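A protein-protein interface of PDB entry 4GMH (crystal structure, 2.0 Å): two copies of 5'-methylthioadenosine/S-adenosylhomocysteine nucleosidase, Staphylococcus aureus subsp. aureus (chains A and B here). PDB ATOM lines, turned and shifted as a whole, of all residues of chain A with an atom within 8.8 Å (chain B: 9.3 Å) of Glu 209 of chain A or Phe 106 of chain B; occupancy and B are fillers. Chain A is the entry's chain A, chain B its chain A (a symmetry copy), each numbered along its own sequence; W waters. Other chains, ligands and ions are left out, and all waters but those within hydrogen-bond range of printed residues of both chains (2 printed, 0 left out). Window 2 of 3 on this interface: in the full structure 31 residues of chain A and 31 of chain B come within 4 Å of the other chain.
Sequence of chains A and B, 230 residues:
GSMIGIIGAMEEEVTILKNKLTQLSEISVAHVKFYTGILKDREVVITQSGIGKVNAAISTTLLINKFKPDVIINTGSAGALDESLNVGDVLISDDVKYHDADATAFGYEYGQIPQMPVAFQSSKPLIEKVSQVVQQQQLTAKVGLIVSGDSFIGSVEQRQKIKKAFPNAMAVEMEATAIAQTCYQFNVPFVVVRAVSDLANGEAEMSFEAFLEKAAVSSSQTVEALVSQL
Glu 12 of chain A touches none of the printed residues of chain B.
Printed residues of chain B within 4 Å of Ile 51 of chain A: Pro 114 (3.8 Å).
Printed residues of chain B within 4 Å of Ser 151 of chain A: Asp 102 (3.4 Å).
Printed residues of chain B within 4 Å of Glu 205 of chain A: Ala 105 (3.5 Å) and Phe 106 (3.9 Å).
Of the printed residues of chain B, Glu 209 of chain A touches Phe 106.
Thr 104 of chain B touches none of the printed residues of chain A.
Of chain A, only Phe 152, Glu 205, Phe 208 and Glu 209 come within 4 Å of Phe 106 of chain B.
OG1 of Thr 104 of chain B is in hydrogen-bond range of OD1 of Asp 102 of chain B.
The side-chain hydroxyl (OG) of Ser 151 of chain A lies within hydrogen-bond range of the backbone NH (N) of Asp 102 of chain B (3.5 Å).
The backbone NH (N) of Phe 152 of chain A is in hydrogen-bond range of the backbone carbonyl oxygen (O) of Asp 102 of chain B (3.1 Å).
Water W1 lies within hydrogen-bond range of O of Pro 114 of chain B (2.8 Å) and N of Ile 51 of chain A (3.1 Å).
Water W2 lies within hydrogen-bond range of N of Ala 105 of chain B, O of Asp 102 of chain B, N of Thr 104 of chain B and O of Phe 152 of chain A.
No position is printed for both chains.
Of the 9 pairs that touch across the chains among the printed residues, none has its exchanged pair printed and touching as well.
Of the 11 printed residues of chain B, 4 touch a printed residue of chain A.
Printed residues of chain B that touch a printed residue of chain A: Asp 102, Ala 105, Phe 106 and Pro 114.
Hydrophobic or aromatic side chains of chain B that line the printed part of chain A: Ala 105, Phe 106 and Pro 114.
Printed residues of chain A that touch a printed residue of chain B: Ile 51, Ser 151, Phe 152, Glu 205, Phe 208 and Glu 209.
Among the printed residues, no Asp or Glu carboxylate lies within 4 Å of a Lys or Arg side-chain nitrogen of the other chain.
Among the printed residues, pairs that only touch across the chains: Glu 205 of chain A with Ala 105 of chain B, Phe 152 of chain A with Phe 106 of chain B, Glu 209 of chain A with Phe 106 of chain B, Ile 51 of chain A with Pro 114 of chain B, Phe 208 of chain A with Phe 106 of chain B, Glu 205 of chain A with Phe 106 of chain B and Phe 152 of chain A with Ala 105 of chain B.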
ATOM      1  N   MET A  10     -30.114  -7.093  18.222  1.00  0.00           N
ATOM      2  CA  MET A  10     -29.769  -7.041  19.668  1.00  0.00           C
ATOM      3  C   MET A  10     -30.941  -6.433  20.530  1.00  0.00           C
ATOM      4  O   MET A  10     -31.717  -5.609  20.016  1.00  0.00           O
ATOM      5  CB  MET A  10     -28.537  -6.116  19.818  1.00  0.00           C
ATOM      6  CG  MET A  10     -27.208  -6.537  19.131  1.00  0.00           C
ATOM      7  SD  MET A  10     -25.860  -5.335  19.506  1.00  0.00           S
ATOM      8  CE  MET A  10     -25.136  -6.092  20.893  1.00  0.00           C
ATOM      9  N   GLU A  12     -30.899  -3.977  22.815  1.00  0.00           N
ATOM     10  CA  GLU A  12     -30.768  -2.500  22.753  1.00  0.00           C
ATOM     11  C   GLU A  12     -31.384  -1.888  21.506  1.00  0.00           C
ATOM     12  O   GLU A  12     -31.789  -0.699  21.530  1.00  0.00           O
ATOM     13  CB  GLU A  12     -29.288  -2.065  22.802  1.00  0.00           C
ATOM     14  CG  GLU A  12     -28.573  -2.367  24.120  1.00  0.00           C
ATOM     15  CD  GLU A  12     -27.926  -3.749  24.179  1.00  0.00           C
ATOM     16  OE1 GLU A  12     -28.281  -4.716  23.405  1.00  0.00           O
ATOM     17  OE2 GLU A  12     -27.001  -3.877  25.018  1.00  0.00           O
ATOM     18  N   ILE A  51     -27.265 -12.172  15.996  1.00  0.00           N
ATOM     19  CA  ILE A  51     -26.186 -11.556  15.150  1.00  0.00           C
ATOM     20  C   ILE A  51     -25.681 -12.425  13.946  1.00  0.00           C
ATOM     21  O   ILE A  51     -25.558 -13.694  14.095  1.00  0.00           O
ATOM     22  CB  ILE A  51     -25.002 -11.094  16.048  1.00  0.00           C
ATOM     23  CG1 ILE A  51     -25.454  -9.917  16.966  1.00  0.00           C
ATOM     24  CG2 ILE A  51     -23.714 -10.666  15.270  1.00  0.00           C
ATOM     25  CD1 ILE A  51     -24.469  -9.672  18.122  1.00  0.00           C
ATOM     26  N   SER A 151     -17.836 -10.653   9.907  1.00  0.00           N
ATOM     27  CA  SER A 151     -16.786 -10.011  10.769  1.00  0.00           C
ATOM     28  C   SER A 151     -17.163  -8.532  11.257  1.00  0.00           C
ATOM     29  O   SER A 151     -17.939  -7.771  10.559  1.00  0.00           O
ATOM     30  CB  SER A 151     -15.446  -9.936   9.991  1.00  0.00           C
ATOM     31  OG  SER A 151     -15.005 -11.207   9.486  1.00  0.00           O
ATOM     32  N   PHE A 152     -16.683  -8.151  12.439  1.00  0.00           N
ATOM     33  CA  PHE A 152     -16.675  -6.767  12.943  1.00  0.00           C
ATOM     34  C   PHE A 152     -15.401  -6.063  12.434  1.00  0.00           C
ATOM     35  O   PHE A 152     -14.262  -6.573  12.614  1.00  0.00           O
ATOM     36  CB  PHE A 152     -16.741  -6.725  14.501  1.00  0.00           C
ATOM     37  CG  PHE A 152     -16.931  -5.301  15.082  1.00  0.00           C
ATOM     38  CD1 PHE A 152     -18.185  -4.670  15.063  1.00  0.00           C
ATOM     39  CD2 PHE A 152     -15.850  -4.594  15.625  1.00  0.00           C
ATOM     40  CE1 PHE A 152     -18.347  -3.371  15.574  1.00  0.00           C
ATOM     41  CE2 PHE A 152     -15.988  -3.285  16.122  1.00  0.00           C
ATOM     42  CZ  PHE A 152     -17.245  -2.666  16.099  1.00  0.00           C
ATOM     43  N   ILE A 153     -15.586  -4.952  11.710  1.00  0.00           N
ATOM     44  CA  ILE A 153     -14.443  -4.236  11.085  1.00  0.00           C
ATOM     45  C   ILE A 153     -13.865  -3.277  12.103  1.00  0.00           C
ATOM     46  O   ILE A 153     -14.438  -2.198  12.343  1.00  0.00           O
ATOM     47  CB  ILE A 153     -14.854  -3.492   9.759  1.00  0.00           C
ATOM     48  CG1 ILE A 153     -15.606  -4.439   8.769  1.00  0.00           C
ATOM     49  CG2 ILE A 153     -13.644  -2.825   9.084  1.00  0.00           C
ATOM     50  CD1 ILE A 153     -14.936  -5.806   8.449  1.00  0.00           C
ATOM     51  N   GLY A 154     -12.816  -3.710  12.821  1.00  0.00           N
ATOM     52  CA  GLY A 154     -12.200  -2.814  13.815  1.00  0.00           C
ATOM     53  C   GLY A 154     -10.713  -2.485  13.722  1.00  0.00           C
ATOM     54  O   GLY A 154     -10.040  -2.418  14.795  1.00  0.00           O
ATOM     55  N   MET A 174     -23.535  -6.499   9.596  1.00  0.00           N
ATOM     56  CA  MET A 174     -23.497  -7.998   9.656  1.00  0.00           C
ATOM     57  C   MET A 174     -24.822  -8.760   9.235  1.00  0.00           C
ATOM     58  O   MET A 174     -24.805 -10.034   9.225  1.00  0.00           O
ATOM     59  CB  MET A 174     -22.981  -8.456  11.091  1.00  0.00           C
ATOM     60  CG  MET A 174     -21.563  -7.904  11.489  1.00  0.00           C
ATOM     61  SD  MET A 174     -20.938  -8.399  13.204  1.00  0.00           S
ATOM     62  CE  MET A 174     -20.551 -10.116  12.909  1.00  0.00           C
ATOM     63  N   SER A 197     -22.730   4.216  14.602  1.00  0.00           N
ATOM     64  CA  SER A 197     -22.221   4.032  15.997  1.00  0.00           C
ATOM     65  C   SER A 197     -20.689   4.221  16.166  1.00  0.00           C
ATOM     66  O   SER A 197     -20.197   4.306  17.312  1.00  0.00           O
ATOM     67  CB  SER A 197     -22.622   2.640  16.594  1.00  0.00           C
ATOM     68  OG  SER A 197     -22.180   1.536  15.763  1.00  0.00           O
ATOM     69  N   ASP A 198     -19.939   4.234  15.044  1.00  0.00           N
ATOM     70  CA  ASP A 198     -18.408   4.125  15.008  1.00  0.00           C
ATOM     71  C   ASP A 198     -17.884   4.365  13.590  1.00  0.00           C
ATOM     72  O   ASP A 198     -18.664   4.313  12.633  1.00  0.00           O
ATOM     73  CB  ASP A 198     -17.887   2.744  15.552  1.00  0.00           C
ATOM     74  CG  ASP A 198     -18.396   1.519  14.702  1.00  0.00           C
ATOM     75  OD1 ASP A 198     -19.522   1.022  14.993  1.00  0.00           O
ATOM     76  OD2 ASP A 198     -17.716   1.107  13.729  1.00  0.00           O
ATOM     77  N   GLU A 203     -10.192   2.733  16.571  1.00  0.00           N
ATOM     78  CA  GLU A 203     -11.077   3.162  17.692  1.00  0.00           C
ATOM     79  C   GLU A 203     -12.481   2.533  17.732  1.00  0.00           C
ATOM     80  O   GLU A 203     -13.306   2.990  18.582  1.00  0.00           O
ATOM     81  CB  GLU A 203     -11.281   4.700  17.687  1.00  0.00           C
ATOM     82  CG  GLU A 203     -10.107   5.515  18.200  1.00  0.00           C
ATOM     83  CD  GLU A 203      -8.942   5.503  17.222  1.00  0.00           C
ATOM     84  OE1 GLU A 203      -9.120   6.068  16.104  1.00  0.00           O
ATOM     85  OE2 GLU A 203      -7.869   4.908  17.570  1.00  0.00           O
ATOM     86  N   ALA A 204     -12.779   1.559  16.824  1.00  0.00           N
ATOM     87  CA  ALA A 204     -14.198   1.099  16.652  1.00  0.00           C
ATOM     88  C   ALA A 204     -14.855   0.476  17.890  1.00  0.00           C
ATOM     89  O   ALA A 204     -16.010   0.739  18.172  1.00  0.00           O
ATOM     90  CB  ALA A 204     -14.328   0.141  15.464  1.00  0.00           C
ATOM     91  N   GLU A 205     -14.121  -0.370  18.613  1.00  0.00           N
ATOM     92  CA  GLU A 205     -14.673  -1.017  19.837  1.00  0.00           C
ATOM     93  C   GLU A 205     -15.024  -0.010  20.988  1.00  0.00           C
ATOM     94  O   GLU A 205     -16.106  -0.120  21.618  1.00  0.00           O
ATOM     95  CB  GLU A 205     -13.718  -2.111  20.304  1.00  0.00           C
ATOM     96  CG  GLU A 205     -14.295  -3.032  21.356  1.00  0.00           C
ATOM     97  CD  GLU A 205     -13.332  -3.236  22.506  1.00  0.00           C
ATOM     98  OE1 GLU A 205     -12.100  -3.193  22.269  1.00  0.00           O
ATOM     99  OE2 GLU A 205     -13.801  -3.455  23.646  1.00  0.00           O
ATOM    100  N   MET A 206     -14.136   0.961  21.246  1.00  0.00           N
ATOM    101  CA  MET A 206     -14.425   2.031  22.268  1.00  0.00           C
ATOM    102  C   MET A 206     -15.571   2.982  21.840  1.00  0.00           C
ATOM    103  O   MET A 206     -16.445   3.307  22.667  1.00  0.00           O
ATOM    104  CB  MET A 206     -13.111   2.800  22.668  1.00  0.00           C
ATOM    105  N   SER A 207     -15.613   3.421  20.558  1.00  0.00           N
ATOM    106  CA  SER A 207     -16.772   4.179  20.030  1.00  0.00           C
ATOM    107  C   SER A 207     -18.147   3.450  20.217  1.00  0.00           C
ATOM    108  O   SER A 207     -19.160   4.069  20.691  1.00  0.00           O
ATOM    109  CB  SER A 207     -16.540   4.575  18.528  1.00  0.00           C
ATOM    110  OG  SER A 207     -17.622   5.346  17.950  1.00  0.00           O
ATOM    111  N   PHE A 208     -18.180   2.147  19.841  1.00  0.00           N
ATOM    112  CA  PHE A 208     -19.403   1.287  19.910  1.00  0.00           C
ATOM    113  C   PHE A 208     -19.910   1.225  21.367  1.00  0.00           C
ATOM    114  O   PHE A 208     -21.095   1.377  21.583  1.00  0.00           O
ATOM    115  CB  PHE A 208     -19.104  -0.191  19.366  1.00  0.00           C
ATOM    116  CG  PHE A 208     -20.356  -1.099  19.230  1.00  0.00           C
ATOM    117  CD1 PHE A 208     -21.163  -1.073  18.066  1.00  0.00           C
ATOM    118  CD2 PHE A 208     -20.707  -1.992  20.258  1.00  0.00           C
ATOM    119  CE1 PHE A 208     -22.309  -1.919  17.952  1.00  0.00           C
ATOM    120  CE2 PHE A 208     -21.845  -2.829  20.160  1.00  0.00           C
ATOM    121  CZ  PHE A 208     -22.650  -2.814  18.999  1.00  0.00           C
ATOM    122  N   GLU A 209     -19.054   0.970  22.362  1.00  0.00           N
ATOM    123  CA  GLU A 209     -19.534   1.000  23.794  1.00  0.00           C
ATOM    124  C   GLU A 209     -20.125   2.358  24.203  1.00  0.00           C
ATOM    125  O   GLU A 209     -21.082   2.420  25.017  1.00  0.00           O
ATOM    126  CB  GLU A 209     -18.416   0.720  24.800  1.00  0.00           C
ATOM    127  CG  GLU A 209     -17.608  -0.520  24.561  1.00  0.00           C
ATOM    128  CD  GLU A 209     -18.436  -1.764  24.731  1.00  0.00           C
ATOM    129  OE1 GLU A 209     -19.312  -1.761  25.648  1.00  0.00           O
ATOM    130  OE2 GLU A 209     -18.200  -2.725  23.944  1.00  0.00           O
ATOM    131  N   ALA A 210     -19.551   3.458  23.691  1.00  0.00           N
ATOM    132  CA  ALA A 210     -20.075   4.804  24.054  1.00  0.00           C
ATOM    133  C   ALA A 210     -21.371   5.235  23.331  1.00  0.00           C
ATOM    134  O   ALA A 210     -22.248   5.985  23.878  1.00  0.00           O
ATOM    135  CB  ALA A 210     -18.970   5.863  23.877  1.00  0.00           C
ATOM    136  N   PHE A 211     -21.501   4.826  22.070  1.00  0.00           N
ATOM    137  CA  PHE A 211     -22.485   5.429  21.213  1.00  0.00           C
ATOM    138  C   PHE A 211     -23.595   4.454  20.689  1.00  0.00           C
ATOM    139  O   PHE A 211     -24.417   4.859  19.869  1.00  0.00           O
ATOM    140  CB  PHE A 211     -21.821   6.260  20.069  1.00  0.00           C
ATOM    141  CG  PHE A 211     -21.006   7.503  20.536  1.00  0.00           C
ATOM    142  CD1 PHE A 211     -21.653   8.630  21.126  1.00  0.00           C
ATOM    143  CD2 PHE A 211     -19.641   7.576  20.292  1.00  0.00           C
ATOM    144  CE1 PHE A 211     -20.920   9.796  21.481  1.00  0.00           C
ATOM    145  CE2 PHE A 211     -18.880   8.716  20.678  1.00  0.00           C
ATOM    146  CZ  PHE A 211     -19.527   9.817  21.280  1.00  0.00           C
ATOM    147  N   LEU A 212     -23.609   3.182  21.123  1.00  0.00           N
ATOM    148  CA  LEU A 212     -24.706   2.252  20.684  1.00  0.00           C
ATOM    149  C   LEU A 212     -26.091   2.819  20.991  1.00  0.00           C
ATOM    150  O   LEU A 212     -26.954   2.831  20.076  1.00  0.00           O
ATOM    151  CB  LEU A 212     -24.580   0.851  21.330  1.00  0.00           C
ATOM    152  CG  LEU A 212     -25.680  -0.187  21.056  1.00  0.00           C
ATOM    153  CD1 LEU A 212     -26.003  -0.363  19.571  1.00  0.00           C
ATOM    154  CD2 LEU A 212     -25.405  -1.541  21.697  1.00  0.00           C
ATOM    155  N   GLU A 213     -26.310   3.346  22.226  1.00  0.00           N
ATOM    156  CA  GLU A 213     -27.637   3.937  22.591  1.00  0.00           C
ATOM    157  C   GLU A 213     -28.069   5.088  21.708  1.00  0.00           C
ATOM    158  O   GLU A 213     -29.215   5.138  21.281  1.00  0.00           O
ATOM    159  CB  GLU A 213     -27.687   4.386  24.076  1.00  0.00           C
ATOM    160  N   LYS A 214     -27.126   5.992  21.408  1.00  0.00           N
ATOM    161  CA  LYS A 214     -27.386   7.175  20.580  1.00  0.00           C
ATOM    162  C   LYS A 214     -27.855   6.804  19.190  1.00  0.00           C
ATOM    163  O   LYS A 214     -28.821   7.383  18.678  1.00  0.00           O
ATOM    164  CB  LYS A 214     -26.129   8.057  20.507  1.00  0.00           C
ATOM    165  CG  LYS A 214     -26.343   9.356  19.721  1.00  0.00           C
ATOM    166  CD  LYS A 214     -25.022  10.050  19.494  1.00  0.00           C
ATOM    167  CE  LYS A 214     -25.150  11.193  18.520  1.00  0.00           C
ATOM    168  NZ  LYS A 214     -25.578  12.465  19.187  1.00  0.00           N
ATOM    169  N   ASP B 102     -15.099 -13.385  12.164  1.00  0.00           N
ATOM    170  CA  ASP B 102     -14.157 -12.628  13.107  1.00  0.00           C
ATOM    171  C   ASP B 102     -14.823 -11.508  14.011  1.00  0.00           C
ATOM    172  O   ASP B 102     -14.955 -10.400  13.566  1.00  0.00           O
ATOM    173  CB  ASP B 102     -12.971 -12.067  12.309  1.00  0.00           C
ATOM    174  CG  ASP B 102     -11.847 -11.406  13.242  1.00  0.00           C
ATOM    175  OD1 ASP B 102     -11.980 -11.472  14.464  1.00  0.00           O
ATOM    176  OD2 ASP B 102     -10.875 -10.845  12.695  1.00  0.00           O
ATOM    177  N   ALA B 103     -15.324 -11.850  15.200  1.00  0.00           N
ATOM    178  CA  ALA B 103     -15.699 -10.871  16.280  1.00  0.00           C
ATOM    179  C   ALA B 103     -14.660 -10.869  17.477  1.00  0.00           C
ATOM    180  O   ALA B 103     -15.068 -10.679  18.665  1.00  0.00           O
ATOM    181  CB  ALA B 103     -17.071 -11.236  16.847  1.00  0.00           C
ATOM    182  N   THR B 104     -13.359 -11.101  17.179  1.00  0.00           N
ATOM    183  CA  THR B 104     -12.338 -11.048  18.266  1.00  0.00           C
ATOM    184  C   THR B 104     -12.145  -9.632  18.922  1.00  0.00           C
ATOM    185  O   THR B 104     -11.703  -9.582  20.084  1.00  0.00           O
ATOM    186  CB  THR B 104     -10.983 -11.603  17.832  1.00  0.00           C
ATOM    187  OG1 THR B 104     -10.477 -10.801  16.772  1.00  0.00           O
ATOM    188  CG2 THR B 104     -11.108 -13.116  17.313  1.00  0.00           C
ATOM    189  N   ALA B 105     -12.473  -8.519  18.233  1.00  0.00           N
ATOM    190  CA  ALA B 105     -12.451  -7.156  18.892  1.00  0.00           C
ATOM    191  C   ALA B 105     -13.240  -7.148  20.191  1.00  0.00           C
ATOM    192  O   ALA B 105     -12.879  -6.422  21.137  1.00  0.00           O
ATOM    193  CB  ALA B 105     -12.973  -6.057  17.983  1.00  0.00           C
ATOM    194  N   PHE B 106     -14.276  -7.972  20.271  1.00  0.00           N
ATOM    195  CA  PHE B 106     -15.023  -8.180  21.541  1.00  0.00           C
ATOM    196  C   PHE B 106     -14.599  -9.335  22.461  1.00  0.00           C
ATOM    197  O   PHE B 106     -15.374  -9.682  23.350  1.00  0.00           O
ATOM    198  CB  PHE B 106     -16.513  -8.303  21.306  1.00  0.00           C
ATOM    199  CG  PHE B 106     -17.094  -7.087  20.634  1.00  0.00           C
ATOM    200  CD1 PHE B 106     -17.255  -5.889  21.340  1.00  0.00           C
ATOM    201  CD2 PHE B 106     -17.426  -7.117  19.291  1.00  0.00           C
ATOM    202  CE1 PHE B 106     -17.780  -4.745  20.704  1.00  0.00           C
ATOM    203  CE2 PHE B 106     -17.926  -5.981  18.658  1.00  0.00           C
ATOM    204  CZ  PHE B 106     -18.099  -4.787  19.364  1.00  0.00           C
ATOM    205  N   GLY B 107     -13.414  -9.924  22.243  1.00  0.00           N
ATOM    206  CA  GLY B 107     -12.946 -11.094  23.035  1.00  0.00           C
ATOM    207  C   GLY B 107     -13.469 -12.516  22.713  1.00  0.00           C
ATOM    208  O   GLY B 107     -13.188 -13.462  23.460  1.00  0.00           O
ATOM    209  N   TYR B 108     -14.284 -12.695  21.671  1.00  0.00           N
ATOM    210  CA  TYR B 108     -14.698 -14.087  21.245  1.00  0.00           C
ATOM    211  C   TYR B 108     -13.567 -14.882  20.572  1.00  0.00           C
ATOM    212  O   TYR B 108     -12.624 -14.268  20.089  1.00  0.00           O
ATOM    213  CB  TYR B 108     -15.879 -13.984  20.269  1.00  0.00           C
ATOM    214  CG  TYR B 108     -17.135 -13.456  20.903  1.00  0.00           C
ATOM    215  CD1 TYR B 108     -17.964 -14.317  21.636  1.00  0.00           C
ATOM    216  CD2 TYR B 108     -17.547 -12.081  20.727  1.00  0.00           C
ATOM    217  CE1 TYR B 108     -19.141 -13.848  22.216  1.00  0.00           C
ATOM    218  CE2 TYR B 108     -18.735 -11.615  21.320  1.00  0.00           C
ATOM    219  CZ  TYR B 108     -19.500 -12.527  22.060  1.00  0.00           C
ATOM    220  OH  TYR B 108     -20.670 -12.185  22.662  1.00  0.00           O
ATOM    221  N   GLU B 109     -13.693 -16.228  20.439  1.00  0.00           N
ATOM    222  CA  GLU B 109     -12.671 -17.051  19.739  1.00  0.00           C
ATOM    223  C   GLU B 109     -12.710 -16.815  18.214  1.00  0.00           C
ATOM    224  O   GLU B 109     -13.769 -16.531  17.686  1.00  0.00           O
ATOM    225  CB  GLU B 109     -12.856 -18.572  19.963  1.00  0.00           C
ATOM    226  CG  GLU B 109     -12.659 -19.130  21.377  1.00  0.00           C
ATOM    227  CD  GLU B 109     -11.317 -18.764  22.019  1.00  0.00           C
ATOM    228  OE1 GLU B 109     -10.267 -19.056  21.422  1.00  0.00           O
ATOM    229  OE2 GLU B 109     -11.297 -18.195  23.135  1.00  0.00           O
ATOM    230  N   GLN B 112     -16.043 -18.033  15.838  1.00  0.00           N
ATOM    231  CA  GLN B 112     -17.268 -18.033  16.676  1.00  0.00           C
ATOM    232  C   GLN B 112     -18.242 -16.819  16.383  1.00  0.00           C
ATOM    233  O   GLN B 112     -17.813 -15.643  16.363  1.00  0.00           O
ATOM    234  CB  GLN B 112     -16.892 -18.010  18.188  1.00  0.00           C
ATOM    235  CG  GLN B 112     -18.019 -18.082  19.268  1.00  0.00           C
ATOM    236  CD  GLN B 112     -17.437 -18.068  20.695  1.00  0.00           C
ATOM    237  OE1 GLN B 112     -16.326 -17.532  20.916  1.00  0.00           O
ATOM    238  NE2 GLN B 112     -18.141 -18.684  21.642  1.00  0.00           N
ATOM    239  N   PRO B 114     -21.103 -14.310  17.732  1.00  0.00           N
ATOM    240  CA  PRO B 114     -21.451 -13.767  19.054  1.00  0.00           C
ATOM    241  C   PRO B 114     -22.659 -14.387  19.700  1.00  0.00           C
ATOM    242  O   PRO B 114     -23.774 -14.414  19.094  1.00  0.00           O
ATOM    243  CB  PRO B 114     -21.710 -12.272  18.751  1.00  0.00           C
ATOM    244  CG  PRO B 114     -20.794 -11.970  17.645  1.00  0.00           C
ATOM    245  CD  PRO B 114     -20.732 -13.230  16.799  1.00  0.00           C
ATOM    246  N   GLN B 115     -22.481 -14.902  20.919  1.00  0.00           N
ATOM    247  CA  GLN B 115     -23.551 -15.570  21.667  1.00  0.00           C
ATOM    248  C   GLN B 115     -23.850 -17.005  21.324  1.00  0.00           C
ATOM    249  O   GLN B 115     -24.736 -17.545  21.932  1.00  0.00           O
ATOM    250  CB  GLN B 115     -24.894 -14.740  21.796  1.00  0.00           C
ATOM    251  CG  GLN B 115     -24.856 -13.474  22.703  1.00  0.00           C
ATOM    252  CD  GLN B 115     -24.570 -13.821  24.233  1.00  0.00           C
ATOM    253  OE1 GLN B 115     -25.508 -14.195  25.002  1.00  0.00           O
ATOM    254  NE2 GLN B 115     -23.260 -13.721  24.675  1.00  0.00           N
HETATM  255  O   HOH W   1     -26.434 -13.781  18.479  1.00  0.00           O
HETATM  256  O   HOH W   2     -13.164  -8.402  15.322  1.00  0.00           O
